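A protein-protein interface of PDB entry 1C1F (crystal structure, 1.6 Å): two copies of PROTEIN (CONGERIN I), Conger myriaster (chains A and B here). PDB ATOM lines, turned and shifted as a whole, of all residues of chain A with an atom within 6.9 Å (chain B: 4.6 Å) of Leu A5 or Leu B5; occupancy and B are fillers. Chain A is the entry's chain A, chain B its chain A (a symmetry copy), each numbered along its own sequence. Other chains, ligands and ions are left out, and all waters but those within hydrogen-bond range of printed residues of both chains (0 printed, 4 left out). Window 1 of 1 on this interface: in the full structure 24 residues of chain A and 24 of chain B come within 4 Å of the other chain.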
ATOM      1  N   GLY A   3      28.674   2.496  28.391  1.00  0.00           N
ATOM      2  CA  GLY A   3      27.525   1.817  28.949  1.00  0.00           C
ATOM      3  C   GLY A   3      27.230   0.664  28.020  1.00  0.00           C
ATOM      4  O   GLY A   3      27.305   0.891  26.815  1.00  0.00           O
ATOM      5  N   GLY A   4      26.951  -0.512  28.539  1.00  0.00           N
ATOM      6  CA  GLY A   4      26.786  -1.670  27.722  1.00  0.00           C
ATOM      7  C   GLY A   4      28.051  -2.501  27.816  1.00  0.00           C
ATOM      8  O   GLY A   4      29.075  -2.085  28.402  1.00  0.00           O
ATOM      9  N   LEU A   5      27.898  -3.697  27.284  1.00  0.00           N
ATOM     10  CA  LEU A   5      28.977  -4.655  27.245  1.00  0.00           C
ATOM     11  C   LEU A   5      29.143  -5.077  25.808  1.00  0.00           C
ATOM     12  O   LEU A   5      28.178  -5.429  25.127  1.00  0.00           O
ATOM     13  CB  LEU A   5      28.644  -5.873  28.103  1.00  0.00           C
ATOM     14  CG  LEU A   5      29.711  -6.957  28.168  1.00  0.00           C
ATOM     15  CD1 LEU A   5      30.932  -6.411  28.879  1.00  0.00           C
ATOM     16  CD2 LEU A   5      29.185  -8.156  28.892  1.00  0.00           C
ATOM     17  N   GLN A   6      30.369  -5.014  25.316  1.00  0.00           N
ATOM     18  CA  GLN A   6      30.711  -5.493  23.999  1.00  0.00           C
ATOM     19  C   GLN A   6      31.151  -6.945  24.169  1.00  0.00           C
ATOM     20  O   GLN A   6      32.120  -7.238  24.883  1.00  0.00           O
ATOM     21  CB  GLN A   6      31.841  -4.626  23.437  1.00  0.00           C
ATOM     22  CG  GLN A   6      32.297  -4.988  22.030  1.00  0.00           C
ATOM     23  CD  GLN A   6      31.197  -4.854  20.971  1.00  0.00           C
ATOM     24  OE1 GLN A   6      31.037  -5.695  20.094  1.00  0.00           O
ATOM     25  NE2 GLN A   6      30.391  -3.814  21.004  1.00  0.00           N
ATOM     26  N   VAL A   7      30.421  -7.858  23.565  1.00  0.00           N
ATOM     27  CA  VAL A   7      30.741  -9.270  23.630  1.00  0.00           C
ATOM     28  C   VAL A   7      31.300  -9.588  22.254  1.00  0.00           C
ATOM     29  O   VAL A   7      30.564  -9.803  21.277  1.00  0.00           O
ATOM     30  CB  VAL A   7      29.466 -10.143  23.912  1.00  0.00           C
ATOM     31  CG1 VAL A   7      29.908 -11.595  24.084  1.00  0.00           C
ATOM     32  CG2 VAL A   7      28.738  -9.704  25.196  1.00  0.00           C
ATOM     33  N   LYS A   8      32.630  -9.645  22.197  1.00  0.00           N
ATOM     34  CA  LYS A   8      33.346  -9.801  20.941  1.00  0.00           C
ATOM     35  C   LYS A   8      32.942 -11.011  20.132  1.00  0.00           C
ATOM     36  O   LYS A   8      32.767 -10.989  18.914  1.00  0.00           O
ATOM     37  CB  LYS A   8      34.852  -9.900  21.180  1.00  0.00           C
ATOM     38  CG  LYS A   8      35.602  -9.740  19.865  1.00  0.00           C
ATOM     39  CD  LYS A   8      36.932 -10.432  19.967  1.00  0.00           C
ATOM     40  CE  LYS A   8      37.637 -10.442  18.616  1.00  0.00           C
ATOM     41  NZ  LYS A   8      38.870 -11.207  18.716  1.00  0.00           N
ATOM     42  N   ASN A   9      32.726 -12.094  20.856  1.00  0.00           N
ATOM     43  CA  ASN A   9      32.463 -13.375  20.237  1.00  0.00           C
ATOM     44  C   ASN A   9      31.104 -13.504  19.592  1.00  0.00           C
ATOM     45  O   ASN A   9      30.877 -14.411  18.801  1.00  0.00           O
ATOM     46  CB  ASN A   9      32.569 -14.498  21.255  1.00  0.00           C
ATOM     47  CG  ASN A   9      33.937 -14.548  21.873  1.00  0.00           C
ATOM     48  OD1 ASN A   9      34.250 -13.701  22.707  1.00  0.00           O
ATOM     49  ND2 ASN A   9      34.736 -15.510  21.474  1.00  0.00           N
ATOM     50  N   PHE A  10      30.184 -12.633  19.950  1.00  0.00           N
ATOM     51  CA  PHE A  10      28.846 -12.804  19.450  1.00  0.00           C
ATOM     52  C   PHE A  10      28.606 -12.057  18.164  1.00  0.00           C
ATOM     53  O   PHE A  10      28.436 -10.862  18.161  1.00  0.00           O
ATOM     54  CB  PHE A  10      27.869 -12.345  20.554  1.00  0.00           C
ATOM     55  CG  PHE A  10      27.606 -13.319  21.703  1.00  0.00           C
ATOM     56  CD1 PHE A  10      28.304 -14.533  21.825  1.00  0.00           C
ATOM     57  CD2 PHE A  10      26.618 -12.992  22.638  1.00  0.00           C
ATOM     58  CE1 PHE A  10      27.985 -15.407  22.869  1.00  0.00           C
ATOM     59  CE2 PHE A  10      26.308 -13.876  23.679  1.00  0.00           C
ATOM     60  CZ  PHE A  10      26.998 -15.086  23.802  1.00  0.00           C
ATOM     61  N   ASP A  11      28.635 -12.655  17.023  1.00  0.00           N
ATOM     62  CA  ASP A  11      28.340 -12.068  15.743  1.00  0.00           C
ATOM     63  C   ASP A  11      26.972 -12.556  15.380  1.00  0.00           C
ATOM     64  O   ASP A  11      26.785 -13.716  15.059  1.00  0.00           O
ATOM     65  CB  ASP A  11      29.316 -12.504  14.647  1.00  0.00           C
ATOM     66  CG  ASP A  11      30.705 -11.916  14.814  1.00  0.00           C
ATOM     67  OD1 ASP A  11      30.803 -10.716  15.056  1.00  0.00           O
ATOM     68  OD2 ASP A  11      31.690 -12.651  14.684  1.00  0.00           O
ATOM     69  N   PHE A  12      26.004 -11.676  15.519  1.00  0.00           N
ATOM     70  CA  PHE A  12      24.632 -12.014  15.226  1.00  0.00           C
ATOM     71  C   PHE A  12      24.403 -11.802  13.743  1.00  0.00           C
ATOM     72  O   PHE A  12      24.024 -10.742  13.245  1.00  0.00           O
ATOM     73  CB  PHE A  12      23.689 -11.135  16.056  1.00  0.00           C
ATOM     74  CG  PHE A  12      22.213 -11.522  15.945  1.00  0.00           C
ATOM     75  CD1 PHE A  12      21.816 -12.858  15.783  1.00  0.00           C
ATOM     76  CD2 PHE A  12      21.246 -10.506  15.999  1.00  0.00           C
ATOM     77  CE1 PHE A  12      20.463 -13.183  15.680  1.00  0.00           C
ATOM     78  CE2 PHE A  12      19.899 -10.850  15.896  1.00  0.00           C
ATOM     79  CZ  PHE A  12      19.503 -12.176  15.729  1.00  0.00           C
ATOM     80  N   LEU A  18      19.802 -15.885  18.476  1.00  0.00           N
ATOM     81  CA  LEU A  18      20.054 -15.068  19.638  1.00  0.00           C
ATOM     82  C   LEU A  18      18.899 -15.241  20.605  1.00  0.00           C
ATOM     83  O   LEU A  18      17.756 -14.927  20.259  1.00  0.00           O
ATOM     84  CB  LEU A  18      20.160 -13.591  19.248  1.00  0.00           C
ATOM     85  CG  LEU A  18      20.334 -12.532  20.357  1.00  0.00           C
ATOM     86  CD1 LEU A  18      21.743 -12.626  20.911  1.00  0.00           C
ATOM     87  CD2 LEU A  18      20.056 -11.132  19.806  1.00  0.00           C
ATOM     88  N   VAL A  35      16.901  -4.762  18.199  1.00  0.00           N
ATOM     89  CA  VAL A  35      18.159  -5.121  17.559  1.00  0.00           C
ATOM     90  C   VAL A  35      18.317  -4.269  16.314  1.00  0.00           C
ATOM     91  O   VAL A  35      17.356  -3.985  15.576  1.00  0.00           O
ATOM     92  CB  VAL A  35      18.261  -6.630  17.139  1.00  0.00           C
ATOM     93  CG1 VAL A  35      18.360  -7.473  18.391  1.00  0.00           C
ATOM     94  CG2 VAL A  35      17.061  -7.087  16.332  1.00  0.00           C
ATOM     95  N   GLY A  36      19.541  -3.829  16.090  1.00  0.00           N
ATOM     96  CA  GLY A  36      19.879  -3.029  14.939  1.00  0.00           C
ATOM     97  C   GLY A  36      21.326  -2.587  15.014  1.00  0.00           C
ATOM     98  O   GLY A  36      22.206  -3.323  15.470  1.00  0.00           O
ATOM     99  N   PHE A 119      24.083  -8.394   9.370  1.00  0.00           N
ATOM    100  CA  PHE A 119      24.838  -8.347  10.604  1.00  0.00           C
ATOM    101  C   PHE A 119      24.151  -7.286  11.456  1.00  0.00           C
ATOM    102  O   PHE A 119      23.802  -6.224  10.922  1.00  0.00           O
ATOM    103  CB  PHE A 119      26.291  -7.937  10.337  1.00  0.00           C
ATOM    104  CG  PHE A 119      27.076  -7.762  11.640  1.00  0.00           C
ATOM    105  CD1 PHE A 119      27.332  -8.871  12.469  1.00  0.00           C
ATOM    106  CD2 PHE A 119      27.520  -6.489  12.025  1.00  0.00           C
ATOM    107  CE1 PHE A 119      28.035  -8.711  13.664  1.00  0.00           C
ATOM    108  CE2 PHE A 119      28.224  -6.343  13.228  1.00  0.00           C
ATOM    109  CZ  PHE A 119      28.474  -7.449  14.047  1.00  0.00           C
ATOM    110  N   LEU A 120      23.910  -7.571  12.734  1.00  0.00           N
ATOM    111  CA  LEU A 120      23.287  -6.600  13.619  1.00  0.00           C
ATOM    112  C   LEU A 120      24.166  -6.434  14.837  1.00  0.00           C
ATOM    113  O   LEU A 120      24.277  -7.377  15.631  1.00  0.00           O
ATOM    114  CB  LEU A 120      21.908  -7.074  14.043  1.00  0.00           C
ATOM    115  CG  LEU A 120      20.922  -7.239  12.883  1.00  0.00           C
ATOM    116  CD1 LEU A 120      19.720  -7.982  13.371  1.00  0.00           C
ATOM    117  CD2 LEU A 120      20.570  -5.880  12.315  1.00  0.00           C
ATOM    118  N   PRO A 121      24.849  -5.297  14.996  1.00  0.00           N
ATOM    119  CA  PRO A 121      25.805  -5.068  16.071  1.00  0.00           C
ATOM    120  C   PRO A 121      25.262  -4.712  17.438  1.00  0.00           C
ATOM    121  O   PRO A 121      26.039  -4.762  18.396  1.00  0.00           O
ATOM    122  CB  PRO A 121      26.698  -3.990  15.522  1.00  0.00           C
ATOM    123  CG  PRO A 121      25.752  -3.159  14.716  1.00  0.00           C
ATOM    124  CD  PRO A 121      24.919  -4.207  14.027  1.00  0.00           C
ATOM    125  N   PHE A 122      23.966  -4.375  17.572  1.00  0.00           N
ATOM    126  CA  PHE A 122      23.425  -3.800  18.781  1.00  0.00           C
ATOM    127  C   PHE A 122      22.133  -4.472  19.245  1.00  0.00           C
ATOM    128  O   PHE A 122      21.223  -4.766  18.461  1.00  0.00           O
ATOM    129  CB  PHE A 122      23.217  -2.301  18.483  1.00  0.00           C
ATOM    130  CG  PHE A 122      22.549  -1.470  19.566  1.00  0.00           C
ATOM    131  CD1 PHE A 122      21.149  -1.377  19.609  1.00  0.00           C
ATOM    132  CD2 PHE A 122      23.339  -0.815  20.515  1.00  0.00           C
ATOM    133  CE1 PHE A 122      20.547  -0.628  20.620  1.00  0.00           C
ATOM    134  CE2 PHE A 122      22.719  -0.070  21.520  1.00  0.00           C
ATOM    135  CZ  PHE A 122      21.331   0.016  21.570  1.00  0.00           C
ATOM    136  N   LEU A 123      22.090  -4.607  20.561  1.00  0.00           N
ATOM    137  CA  LEU A 123      20.955  -5.173  21.259  1.00  0.00           C
ATOM    138  C   LEU A 123      20.616  -4.349  22.489  1.00  0.00           C
ATOM    139  O   LEU A 123      21.502  -3.994  23.285  1.00  0.00           O
ATOM    140  CB  LEU A 123      21.253  -6.641  21.700  1.00  0.00           C
ATOM    141  CG  LEU A 123      20.284  -7.314  22.689  1.00  0.00           C
ATOM    142  CD1 LEU A 123      18.926  -7.493  22.026  1.00  0.00           C
ATOM    143  CD2 LEU A 123      20.819  -8.661  23.133  1.00  0.00           C
ATOM    144  N   VAL A 134      21.926 -13.388  27.626  1.00  0.00           N
ATOM    145  CA  VAL A 134      22.030 -13.349  26.195  1.00  0.00           C
ATOM    146  C   VAL A 134      22.775 -14.636  25.838  1.00  0.00           C
ATOM    147  O   VAL A 134      23.811 -14.962  26.416  1.00  0.00           O
ATOM    148  CB  VAL A 134      22.813 -12.095  25.759  1.00  0.00           C
ATOM    149  CG1 VAL A 134      22.801 -12.028  24.251  1.00  0.00           C
ATOM    150  CG2 VAL A 134      22.145 -10.812  26.249  1.00  0.00           C
ATOM    151  N   LEU A 136      23.898 -17.063  22.324  1.00  0.00           N
ATOM    152  CA  LEU A 136      23.978 -17.032  20.886  1.00  0.00           C
ATOM    153  C   LEU A 136      24.463 -18.420  20.491  1.00  0.00           C
ATOM    154  O   LEU A 136      25.394 -18.943  21.100  1.00  0.00           O
ATOM    155  CB  LEU A 136      24.963 -15.980  20.410  1.00  0.00           C
ATOM    156  CG  LEU A 136      24.977 -15.791  18.889  1.00  0.00           C
ATOM    157  CD1 LEU A 136      23.830 -14.887  18.486  1.00  0.00           C
ATOM    158  CD2 LEU A 136      26.297 -15.193  18.443  1.00  0.00           C
ATOM    159  N   GLY B   3      32.045  -6.551  14.485  1.00  0.00           N
ATOM    160  CA  GLY B   3      32.136  -7.903  14.991  1.00  0.00           C
ATOM    161  C   GLY B   3      31.878  -7.809  16.477  1.00  0.00           C
ATOM    162  O   GLY B   3      32.408  -6.875  17.072  1.00  0.00           O
ATOM    163  N   GLY B   4      31.083  -8.695  17.038  1.00  0.00           N
ATOM    164  CA  GLY B   4      30.699  -8.591  18.408  1.00  0.00           C
ATOM    165  C   GLY B   4      29.285  -8.046  18.464  1.00  0.00           C
ATOM    166  O   GLY B   4      28.693  -7.632  17.442  1.00  0.00           O
ATOM    167  N   LEU B   5      28.765  -8.139  19.672  1.00  0.00           N
ATOM    168  CA  LEU B   5      27.434  -7.667  19.966  1.00  0.00           C
ATOM    169  C   LEU B   5      27.550  -6.705  21.120  1.00  0.00           C
ATOM    170  O   LEU B   5      28.179  -6.997  22.137  1.00  0.00           O
ATOM    171  CB  LEU B   5      26.526  -8.830  20.356  1.00  0.00           C
ATOM    172  CG  LEU B   5      25.080  -8.473  20.672  1.00  0.00           C
ATOM    173  CD1 LEU B   5      24.405  -7.973  19.413  1.00  0.00           C
ATOM    174  CD2 LEU B   5      24.358  -9.671  21.204  1.00  0.00           C
ATOM    175  N   GLN B   6      26.970  -5.527  20.960  1.00  0.00           N
ATOM    176  CA  GLN B   6      26.891  -4.544  22.013  1.00  0.00           C
ATOM    177  C   GLN B   6      25.566  -4.788  22.733  1.00  0.00           C
ATOM    178  O   GLN B   6      24.488  -4.705  22.128  1.00  0.00           O
ATOM    179  CB  GLN B   6      26.940  -3.146  21.388  1.00  0.00           C
ATOM    180  CG  GLN B   6      26.897  -1.991  22.379  1.00  0.00           C
ATOM    181  CD  GLN B   6      28.076  -1.976  23.360  1.00  0.00           C
ATOM    182  OE1 GLN B   6      27.923  -1.735  24.552  1.00  0.00           O
ATOM    183  NE2 GLN B   6      29.288  -2.236  22.918  1.00  0.00           N
ATOM    184  N   VAL B   7      25.638  -5.138  23.999  1.00  0.00           N
ATOM    185  CA  VAL B   7      24.456  -5.381  24.802  1.00  0.00           C
ATOM    186  C   VAL B   7      24.366  -4.165  25.706  1.00  0.00           C
ATOM    187  O   VAL B   7      25.043  -4.062  26.743  1.00  0.00           O
ATOM    188  CB  VAL B   7      24.596  -6.688  25.662  1.00  0.00           C
ATOM    189  CG1 VAL B   7      23.269  -6.932  26.379  1.00  0.00           C
ATOM    190  CG2 VAL B   7      24.910  -7.920  24.794  1.00  0.00           C
ATOM    191  N   PHE B  10      23.851  -4.248  29.650  1.00  0.00           N
ATOM    192  CA  PHE B  10      24.781  -4.860  30.561  1.00  0.00           C
ATOM    193  C   PHE B  10      25.894  -3.931  30.968  1.00  0.00           C
ATOM    194  O   PHE B  10      26.812  -3.693  30.220  1.00  0.00           O
ATOM    195  CB  PHE B  10      25.334  -6.133  29.883  1.00  0.00           C
ATOM    196  CG  PHE B  10      24.443  -7.375  29.897  1.00  0.00           C
ATOM    197  CD1 PHE B  10      23.128  -7.343  30.394  1.00  0.00           C
ATOM    198  CD2 PHE B  10      24.974  -8.579  29.421  1.00  0.00           C
ATOM    199  CE1 PHE B  10      22.377  -8.522  30.427  1.00  0.00           C
ATOM    200  CE2 PHE B  10      24.211  -9.753  29.460  1.00  0.00           C
ATOM    201  CZ  PHE B  10      22.905  -9.727  29.957  1.00  0.00           C
ATOM    202  N   LEU B  18      28.917 -11.199  36.474  1.00  0.00           N
ATOM    203  CA  LEU B  18      28.894 -11.577  35.082  1.00  0.00           C
ATOM    204  C   LEU B  18      29.185 -13.062  34.984  1.00  0.00           C
ATOM    205  O   LEU B  18      30.261 -13.505  35.397  1.00  0.00           O
ATOM    206  CB  LEU B  18      29.958 -10.808  34.295  1.00  0.00           C
ATOM    207  CG  LEU B  18      30.167 -11.132  32.800  1.00  0.00           C
ATOM    208  CD1 LEU B  18      28.993 -10.586  32.009  1.00  0.00           C
ATOM    209  CD2 LEU B  18      31.486 -10.535  32.304  1.00  0.00           C
ATOM    210  N   LEU B 120      33.883  -2.098  33.086  1.00  0.00           N
ATOM    211  CA  LEU B 120      34.630  -2.833  32.077  1.00  0.00           C
ATOM    212  C   LEU B 120      33.740  -3.018  30.868  1.00  0.00           C
ATOM    213  O   LEU B 120      32.752  -3.757  30.957  1.00  0.00           O
ATOM    214  CB  LEU B 120      35.055  -4.189  32.612  1.00  0.00           C
ATOM    215  CG  LEU B 120      35.993  -4.115  33.820  1.00  0.00           C
ATOM    216  CD1 LEU B 120      36.100  -5.474  34.434  1.00  0.00           C
ATOM    217  CD2 LEU B 120      37.338  -3.568  33.389  1.00  0.00           C
ATOM    218  N   PRO B 121      34.008  -2.331  29.754  1.00  0.00           N
ATOM    219  CA  PRO B 121      33.162  -2.350  28.568  1.00  0.00           C
ATOM    220  C   PRO B 121      33.271  -3.537  27.637  1.00  0.00           C
ATOM    221  O   PRO B 121      32.395  -3.678  26.779  1.00  0.00           O
ATOM    222  CB  PRO B 121      33.503  -1.060  27.876  1.00  0.00           C
ATOM    223  CG  PRO B 121      34.961  -0.907  28.166  1.00  0.00           C
ATOM    224  CD  PRO B 121      35.039  -1.308  29.615  1.00  0.00           C
ATOM    225  N   PHE B 122      34.292  -4.403  27.781  1.00  0.00           N
ATOM    226  CA  PHE B 122      34.603  -5.418  26.803  1.00  0.00           C
ATOM    227  C   PHE B 122      34.825  -6.801  27.415  1.00  0.00           C
ATOM    228  O   PHE B 122      35.493  -6.969  28.442  1.00  0.00           O
ATOM    229  CB  PHE B 122      35.853  -4.917  26.052  1.00  0.00           C
ATOM    230  CG  PHE B 122      36.464  -5.858  25.026  1.00  0.00           C
ATOM    231  CD1 PHE B 122      37.420  -6.803  25.430  1.00  0.00           C
ATOM    232  CD2 PHE B 122      36.058  -5.777  23.691  1.00  0.00           C
ATOM    233  CE1 PHE B 122      37.958  -7.675  24.483  1.00  0.00           C
ATOM    234  CE2 PHE B 122      36.607  -6.657  22.758  1.00  0.00           C
ATOM    235  CZ  PHE B 122      37.548  -7.602  23.157  1.00  0.00           C
ATOM    236  N   LEU B 123      34.296  -7.762  26.674  1.00  0.00           N
ATOM    237  CA  LEU B 123      34.405  -9.166  27.009  1.00  0.00           C
ATOM    238  C   LEU B 123      34.745  -9.987  25.778  1.00  0.00           C
ATOM    239  O   LEU B 123      34.129  -9.826  24.711  1.00  0.00           O
ATOM    240  CB  LEU B 123      33.067  -9.695  27.615  1.00  0.00           C
ATOM    241  CG  LEU B 123      32.892 -11.217  27.776  1.00  0.00           C
ATOM    242  CD1 LEU B 123      33.887 -11.735  28.804  1.00  0.00           C
ATOM    243  CD2 LEU B 123      31.480 -11.552  28.214  1.00  0.00           C
ATOM    244  N   VAL B 134      25.989 -15.240  28.133  1.00  0.00           N
ATOM    245  CA  VAL B 134      26.453 -14.188  28.992  1.00  0.00           C
ATOM    246  C   VAL B 134      25.229 -13.821  29.832  1.00  0.00           C
ATOM    247  O   VAL B 134      24.133 -13.610  29.314  1.00  0.00           O
ATOM    248  CB  VAL B 134      26.945 -12.996  28.146  1.00  0.00           C
ATOM    249  CG1 VAL B 134      27.530 -11.963  29.077  1.00  0.00           C
ATOM    250  CG2 VAL B 134      28.069 -13.403  27.196  1.00  0.00           C
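Leu A5 touches just these residues of chain B: Leu B5, Gln B6, Val B7, Phe B10, Leu B18, Leu B120 and Pro B121. Val A35 touches none of the printed residues of chain B. Of the printed residues of chain B, Phe A119 touches Gly B3 (3.7 Å) and Gly B4 (3.4 Å). Of the printed residues of chain B, Pro A121 touches Leu B5 and Gln B6. Of chain A, only Leu A5, Gln A6, Val A7, Phe A10, Leu A18, Leu A120 and Pro A121 come within 4 Å of Leu B5. The nearest residue of chain B that does not touch Leu A5 is Phe B122 (4.1 Å). The nearest printed residue of chain A that does not touch Leu B18 is Val A7 (6.9 Å).
The backbone carbonyl oxygen (O) of Gly A36 is in hydrogen-bond range of the backbone NH (N) of Phe A122. O of Phe A12 lies within hydrogen-bond range of N of Leu A120 (3.2 Å).
The backbone carbonyl oxygen of Phe B10 is in hydrogen-bond range of the backbone NH of Leu A5. O of Pro A121 lies within hydrogen-bond range of N of Gln B6 (2.8 Å). O of Phe A10 lies close to O of Gly B4 (3.3 Å). The backbone carbonyl oxygen of Lys A8 lies close to the backbone NH of Gly B4 (3.4 Å). The side-chain amide oxygen (OE1) of Gln A6 sits at hydrogen-bond distance from the backbone NH (N) of Leu B5. The backbone NH (N) of Leu A5 lies within hydrogen-bond range of the side-chain amide oxygen (OE1) of Gln B6. The backbone carbonyl oxygen of Leu A5 is in hydrogen-bond range of the backbone NH of Val B7, 2.8 Å away. The side-chain carboxylate (OD1) of Asp A11 lies within hydrogen-bond range of the backbone NH (N) of Gly B4 (2.8 Å). The backbone carbonyl oxygen (O) of Gly A4 sits close to the backbone carbonyl oxygen (O) of Phe B10 (3.3 Å). O of Phe A10 is in hydrogen-bond range of N of Leu B5 (3.1 Å). The backbone NH (N) of Leu A123 lies within hydrogen-bond range of the backbone carbonyl oxygen (O) of Gln B6, 2.9 Å away. The backbone NH (N) of Leu B123 lies within hydrogen-bond range of the backbone carbonyl oxygen (O) of Gln A6 (2.9 Å). The backbone carbonyl oxygen of Leu B5 sits close to the backbone carbonyl oxygen of Leu A5. The backbone NH (N) of Val A134 is in hydrogen-bond range of the backbone carbonyl oxygen (O) of Val B134 (2.8 Å). The side-chain amide nitrogen of Gln A6 lies close to the side-chain amide nitrogen of Gln B6, 2.7 Å away. The backbone NH of Gln A6 sits at hydrogen-bond distance from the backbone carbonyl oxygen of Pro B121. N of Val A7 is in hydrogen-bond range of O of Leu B5. The backbone carbonyl oxygen (O) of Leu B123 lies within hydrogen-bond range of the backbone NH (N) of Lys A8 (2.9 Å).
Of the 12 printed residues of chain B, 12 touch a printed residue of chain A. Hydrophobic or aromatic side chains of chain B that line the printed part of chain A: Leu B5, Val B7, Phe B10, Leu B18, Leu B123 and Val B134. Of the 20 printed residues of chain A, 15 touch a printed residue of chain B. Among the printed residues, no Asp or Glu carboxylate lies within 4 Å of a Lys or Arg side-chain nitrogen of the other chain.
Gly A3 touches Gln B6, and with the chains exchanged Gln A6 touches Gly B3. Leu B5 touches its own counterpart, Leu A5. Gln B6 touches its own counterpart, Gln A6. Val A134 touches its own counterpart, Val B134. Positions printed for both chains: 3, 4, 5, 6, 7, 10, 18, 120, 121, 122, 123 and 134.
Among the printed residues, pairs that only touch across the chains: Asp A11 with Gly B3, Gly A4 with Val B7, Val A7 with Gly B4, Gln A6 with Gly B4, Gly A4 with Gln B6, Phe A119 with Gly B4, Gly A3 with Gln B6, Gln A6 with Gly B3, Pro A121 with Leu B5, Leu A5 with Pro B121, Leu A123 with Val B7, Val A7 with Leu B123, Phe A122 with Gln B6, Gln A6 with Phe B122, Phe A119 with Gly B3, Leu A5 with Leu B120, Leu A120 with Leu B5, Phe A10 with Val B134, Val A134 with Phe B10, Leu A18 with Leu B5 and Leu A5 with Leu B18.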
